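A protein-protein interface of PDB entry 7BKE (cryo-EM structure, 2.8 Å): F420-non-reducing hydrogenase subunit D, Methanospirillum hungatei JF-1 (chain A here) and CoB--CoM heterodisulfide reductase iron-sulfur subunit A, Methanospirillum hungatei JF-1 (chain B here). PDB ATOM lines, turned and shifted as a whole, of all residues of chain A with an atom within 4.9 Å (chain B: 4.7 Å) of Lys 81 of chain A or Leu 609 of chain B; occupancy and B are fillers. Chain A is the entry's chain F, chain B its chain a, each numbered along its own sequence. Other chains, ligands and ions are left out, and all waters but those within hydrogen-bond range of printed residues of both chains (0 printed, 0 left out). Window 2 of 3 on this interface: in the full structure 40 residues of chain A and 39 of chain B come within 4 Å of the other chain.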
ATOM      1  N   GLU A  77     -17.706  15.056 -20.260  1.00  0.00           N
ATOM      2  CA  GLU A  77     -17.352  14.644 -21.610  1.00  0.00           C
ATOM      3  C   GLU A  77     -15.972  15.120 -22.030  1.00  0.00           C
ATOM      4  O   GLU A  77     -15.727  15.349 -23.212  1.00  0.00           O
ATOM      5  CB  GLU A  77     -18.399  15.135 -22.589  1.00  0.00           C
ATOM      6  CG  GLU A  77     -18.514  16.624 -22.652  1.00  0.00           C
ATOM      7  CD  GLU A  77     -19.778  17.054 -23.346  1.00  0.00           C
ATOM      8  OE1 GLU A  77     -20.644  16.181 -23.559  1.00  0.00           O
ATOM      9  OE2 GLU A  77     -19.909  18.251 -23.685  1.00  0.00           O
ATOM     10  N   GLY A  78     -15.050  15.250 -21.098  1.00  0.00           N
ATOM     11  CA  GLY A  78     -13.769  15.797 -21.466  1.00  0.00           C
ATOM     12  C   GLY A  78     -12.835  14.855 -22.169  1.00  0.00           C
ATOM     13  O   GLY A  78     -11.813  15.306 -22.684  1.00  0.00           O
ATOM     14  N   ASN A  79     -13.131  13.562 -22.204  1.00  0.00           N
ATOM     15  CA  ASN A  79     -12.221  12.656 -22.885  1.00  0.00           C
ATOM     16  C   ASN A  79     -12.649  12.361 -24.311  1.00  0.00           C
ATOM     17  O   ASN A  79     -11.850  11.837 -25.086  1.00  0.00           O
ATOM     18  CB  ASN A  79     -12.057  11.349 -22.107  1.00  0.00           C
ATOM     19  CG  ASN A  79     -13.352  10.681 -21.805  1.00  0.00           C
ATOM     20  OD1 ASN A  79     -14.417  11.233 -22.020  1.00  0.00           O
ATOM     21  ND2 ASN A  79     -13.275   9.474 -21.300  1.00  0.00           N
ATOM     22  N   TYR A  80     -13.872  12.721 -24.691  1.00  0.00           N
ATOM     23  CA  TYR A  80     -14.224  12.724 -26.105  1.00  0.00           C
ATOM     24  C   TYR A  80     -13.391  13.739 -26.867  1.00  0.00           C
ATOM     25  O   TYR A  80     -12.898  13.458 -27.968  1.00  0.00           O
ATOM     26  CB  TYR A  80     -15.697  13.047 -26.267  1.00  0.00           C
ATOM     27  CG  TYR A  80     -16.630  12.091 -25.596  1.00  0.00           C
ATOM     28  CD1 TYR A  80     -16.576  10.742 -25.857  1.00  0.00           C
ATOM     29  CD2 TYR A  80     -17.590  12.545 -24.724  1.00  0.00           C
ATOM     30  CE1 TYR A  80     -17.445   9.873 -25.254  1.00  0.00           C
ATOM     31  CE2 TYR A  80     -18.460  11.682 -24.120  1.00  0.00           C
ATOM     32  CZ  TYR A  80     -18.383  10.351 -24.387  1.00  0.00           C
ATOM     33  OH  TYR A  80     -19.254   9.492 -23.777  1.00  0.00           O
ATOM     34  N   LYS A  81     -13.225  14.930 -26.297  1.00  0.00           N
ATOM     35  CA  LYS A  81     -12.375  15.937 -26.912  1.00  0.00           C
ATOM     36  C   LYS A  81     -10.952  15.439 -27.039  1.00  0.00           C
ATOM     37  O   LYS A  81     -10.313  15.616 -28.080  1.00  0.00           O
ATOM     38  CB  LYS A  81     -12.421  17.221 -26.093  1.00  0.00           C
ATOM     39  CG  LYS A  81     -13.606  18.093 -26.393  1.00  0.00           C
ATOM     40  CD  LYS A  81     -14.798  17.709 -25.575  1.00  0.00           C
ATOM     41  CE  LYS A  81     -15.902  18.699 -25.787  1.00  0.00           C
ATOM     42  NZ  LYS A  81     -17.082  18.418 -24.956  1.00  0.00           N
ATOM     43  N   ALA A  82     -10.440  14.793 -25.995  1.00  0.00           N
ATOM     44  CA  ALA A  82      -9.092  14.258 -26.054  1.00  0.00           C
ATOM     45  C   ALA A  82      -8.980  13.161 -27.098  1.00  0.00           C
ATOM     46  O   ALA A  82      -7.978  13.081 -27.801  1.00  0.00           O
ATOM     47  CB  ALA A  82      -8.672  13.738 -24.689  1.00  0.00           C
ATOM     48  N   ALA A  83      -9.993  12.305 -27.214  1.00  0.00           N
ATOM     49  CA  ALA A  83      -9.942  11.232 -28.198  1.00  0.00           C
ATOM     50  C   ALA A  83      -9.897  11.781 -29.614  1.00  0.00           C
ATOM     51  O   ALA A  83      -9.109  11.313 -30.441  1.00  0.00           O
ATOM     52  CB  ALA A  83     -11.134  10.300 -28.026  1.00  0.00           C
ATOM     53  N   LYS A  84     -10.736  12.771 -29.916  1.00  0.00           N
ATOM     54  CA  LYS A  84     -10.676  13.389 -31.237  1.00  0.00           C
ATOM     55  C   LYS A  84      -9.318  14.027 -31.482  1.00  0.00           C
ATOM     56  O   LYS A  84      -8.729  13.870 -32.561  1.00  0.00           O
ATOM     57  CB  LYS A  84     -11.784  14.425 -31.377  1.00  0.00           C
ATOM     58  CG  LYS A  84     -12.189  14.718 -32.796  1.00  0.00           C
ATOM     59  CD  LYS A  84     -13.582  15.297 -32.850  1.00  0.00           C
ATOM     60  CE  LYS A  84     -14.002  15.561 -34.273  1.00  0.00           C
ATOM     61  NZ  LYS A  84     -15.310  16.252 -34.350  1.00  0.00           N
ATOM     62  N   ARG A  85      -8.790  14.728 -30.480  1.00  0.00           N
ATOM     63  CA  ARG A  85      -7.487  15.352 -30.641  1.00  0.00           C
ATOM     64  C   ARG A  85      -6.407  14.319 -30.918  1.00  0.00           C
ATOM     65  O   ARG A  85      -5.545  14.537 -31.767  1.00  0.00           O
ATOM     66  CB  ARG A  85      -7.143  16.169 -29.404  1.00  0.00           C
ATOM     67  CG  ARG A  85      -7.618  17.588 -29.465  1.00  0.00           C
ATOM     68  CD  ARG A  85      -7.568  18.245 -28.113  1.00  0.00           C
ATOM     69  NE  ARG A  85      -8.759  19.050 -27.872  1.00  0.00           N
ATOM     70  CZ  ARG A  85      -9.049  19.622 -26.713  1.00  0.00           C
ATOM     71  NH1 ARG A  85      -8.234  19.483 -25.687  1.00  0.00           N
ATOM     72  NH2 ARG A  85     -10.154  20.330 -26.582  1.00  0.00           N
ATOM     73  N   MET B 605     -15.498  29.727 -30.444  1.00  0.00           N
ATOM     74  CA  MET B 605     -15.464  28.298 -30.707  1.00  0.00           C
ATOM     75  C   MET B 605     -15.330  27.477 -29.435  1.00  0.00           C
ATOM     76  O   MET B 605     -15.806  26.339 -29.390  1.00  0.00           O
ATOM     77  CB  MET B 605     -14.333  27.986 -31.686  1.00  0.00           C
ATOM     78  CG  MET B 605     -14.618  28.485 -33.091  1.00  0.00           C
ATOM     79  SD  MET B 605     -13.470  27.952 -34.366  1.00  0.00           S
ATOM     80  CE  MET B 605     -11.918  27.982 -33.501  1.00  0.00           C
ATOM     81  N   CYS B 606     -14.708  28.032 -28.398  1.00  0.00           N
ATOM     82  CA  CYS B 606     -14.586  27.345 -27.120  1.00  0.00           C
ATOM     83  C   CYS B 606     -15.909  27.213 -26.389  1.00  0.00           C
ATOM     84  O   CYS B 606     -16.022  26.372 -25.499  1.00  0.00           O
ATOM     85  CB  CYS B 606     -13.609  28.095 -26.228  1.00  0.00           C
ATOM     86  SG  CYS B 606     -14.073  29.808 -25.959  1.00  0.00           S
ATOM     87  N   VAL B 607     -16.904  28.021 -26.742  1.00  0.00           N
ATOM     88  CA  VAL B 607     -18.128  28.096 -25.948  1.00  0.00           C
ATOM     89  C   VAL B 607     -18.825  26.744 -25.878  1.00  0.00           C
ATOM     90  O   VAL B 607     -19.379  26.370 -24.841  1.00  0.00           O
ATOM     91  CB  VAL B 607     -19.046  29.191 -26.509  1.00  0.00           C
ATOM     92  CG1 VAL B 607     -20.424  29.055 -25.955  1.00  0.00           C
ATOM     93  CG2 VAL B 607     -18.491  30.539 -26.163  1.00  0.00           C
ATOM     94  N   ASN B 608     -18.799  25.988 -26.964  1.00  0.00           N
ATOM     95  CA  ASN B 608     -19.486  24.707 -27.009  1.00  0.00           C
ATOM     96  C   ASN B 608     -18.664  23.564 -26.444  1.00  0.00           C
ATOM     97  O   ASN B 608     -19.146  22.433 -26.421  1.00  0.00           O
ATOM     98  CB  ASN B 608     -19.874  24.381 -28.442  1.00  0.00           C
ATOM     99  CG  ASN B 608     -20.641  25.494 -29.087  1.00  0.00           C
ATOM    100  OD1 ASN B 608     -20.065  26.356 -29.744  1.00  0.00           O
ATOM    101  ND2 ASN B 608     -21.949  25.501 -28.887  1.00  0.00           N
ATOM    102  N   LEU B 609     -17.444  23.814 -25.999  1.00  0.00           N
ATOM    103  CA  LEU B 609     -16.636  22.759 -25.424  1.00  0.00           C
ATOM    104  C   LEU B 609     -16.834  22.601 -23.928  1.00  0.00           C
ATOM    105  O   LEU B 609     -16.209  21.726 -23.332  1.00  0.00           O
ATOM    106  CB  LEU B 609     -15.164  23.008 -25.711  1.00  0.00           C
ATOM    107  CG  LEU B 609     -14.749  22.975 -27.170  1.00  0.00           C
ATOM    108  CD1 LEU B 609     -13.279  22.866 -27.214  1.00  0.00           C
ATOM    109  CD2 LEU B 609     -15.370  21.812 -27.881  1.00  0.00           C
ATOM    110  N   CYS B 610     -17.667  23.422 -23.304  1.00  0.00           N
ATOM    111  CA  CYS B 610     -17.865  23.330 -21.871  1.00  0.00           C
ATOM    112  C   CYS B 610     -19.108  22.519 -21.582  1.00  0.00           C
ATOM    113  O   CYS B 610     -20.201  22.907 -22.015  1.00  0.00           O
ATOM    114  CB  CYS B 610     -17.987  24.712 -21.250  1.00  0.00           C
ATOM    115  SG  CYS B 610     -18.092  24.681 -19.463  1.00  0.00           S
ATOM    116  N   PRO B 611     -18.997  21.389 -20.883  1.00  0.00           N
ATOM    117  CA  PRO B 611     -20.204  20.654 -20.503  1.00  0.00           C
ATOM    118  C   PRO B 611     -21.089  21.422 -19.551  1.00  0.00           C
ATOM    119  O   PRO B 611     -22.300  21.181 -19.505  1.00  0.00           O
ATOM    120  CB  PRO B 611     -19.648  19.385 -19.849  1.00  0.00           C
ATOM    121  CG  PRO B 611     -18.207  19.371 -20.153  1.00  0.00           C
ATOM    122  CD  PRO B 611     -17.780  20.754 -20.367  1.00  0.00           C
ATOM    123  N   THR B 638     -10.721  21.547 -20.791  1.00  0.00           N
ATOM    124  CA  THR B 638     -10.998  21.286 -22.195  1.00  0.00           C
ATOM    125  C   THR B 638     -10.882  22.555 -23.024  1.00  0.00           C
ATOM    126  O   THR B 638     -10.218  22.574 -24.065  1.00  0.00           O
ATOM    127  CB  THR B 638     -12.386  20.676 -22.331  1.00  0.00           C
ATOM    128  OG1 THR B 638     -12.452  19.484 -21.551  1.00  0.00           O
ATOM    129  CG2 THR B 638     -12.666  20.336 -23.749  1.00  0.00           C
ATOM    130  N   PHE B 642      -8.096  23.613 -25.874  1.00  0.00           N
ATOM    131  CA  PHE B 642      -8.515  23.886 -27.240  1.00  0.00           C
ATOM    132  C   PHE B 642      -7.947  25.194 -27.779  1.00  0.00           C
ATOM    133  O   PHE B 642      -7.296  25.200 -28.825  1.00  0.00           O
ATOM    134  CB  PHE B 642     -10.032  23.927 -27.342  1.00  0.00           C
ATOM    135  CG  PHE B 642     -10.516  24.484 -28.633  1.00  0.00           C
ATOM    136  CD1 PHE B 642     -10.395  23.762 -29.795  1.00  0.00           C
ATOM    137  CD2 PHE B 642     -11.059  25.740 -28.696  1.00  0.00           C
ATOM    138  CE1 PHE B 642     -10.820  24.277 -30.987  1.00  0.00           C
ATOM    139  CE2 PHE B 642     -11.491  26.253 -29.887  1.00  0.00           C
ATOM    140  CZ  PHE B 642     -11.372  25.519 -31.029  1.00  0.00           C
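Of the 9 printed residues of chain B, 4 touch a printed residue of chain A.
Among the printed residues, 6 pairs touch across the chains.
Among the printed residues, no Asp or Glu carboxylate lies within 4 Å of a Lys or Arg side-chain nitrogen of the other chain.
The backbone carbonyl oxygen (O) of Thr 638 of chain B is in hydrogen-bond range of the guanidinium group (NH2) of Arg 85 of chain A, at 3.4 Å.
Of the printed residues of chain B, Gly 78 of chain A touches Thr 638.
Of chain B, only Leu 609 (3.8 Å) and Thr 638 (3.6 Å) come within 4 Å of Lys 81 of chain A.
Of the printed residues of chain B, Arg 85 of chain A touches Thr 638 and Phe 642.
Of the printed residues of chain A, Pro 611 of chain B touches Glu 77 (3.7 Å).
Of the printed residues of chain A, Thr 638 of chain B touches Gly 78 (3.9 Å), Lys 81 (3.6 Å) and Arg 85 (3.4 Å).
Of the printed residues of chain A, Phe 642 of chain B touches Arg 85.
The nearest residue of chain A that does not touch Leu 609 of chain B is Arg 85 of chain A (4.1 Å).
The side-chain amino group (NZ) of Lys 81 of chain A lies within salt-bridge range of the side-chain carboxylate (OE2) of Glu 77 of chain A (3.1 Å).
Glu 77 of chain A touches Pro 611 of chain B.
Thr 638 of chain B touches Gly 78 of chain A.
NZ of Lys 81 of chain A touches O of Leu 609 of chain B (3.8 Å).
Lys 81 of chain A touches Thr 638 of chain B.
NH2 of Arg 85 of chain A touches CB of Phe 642 of chain B, 3.7 Å away.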
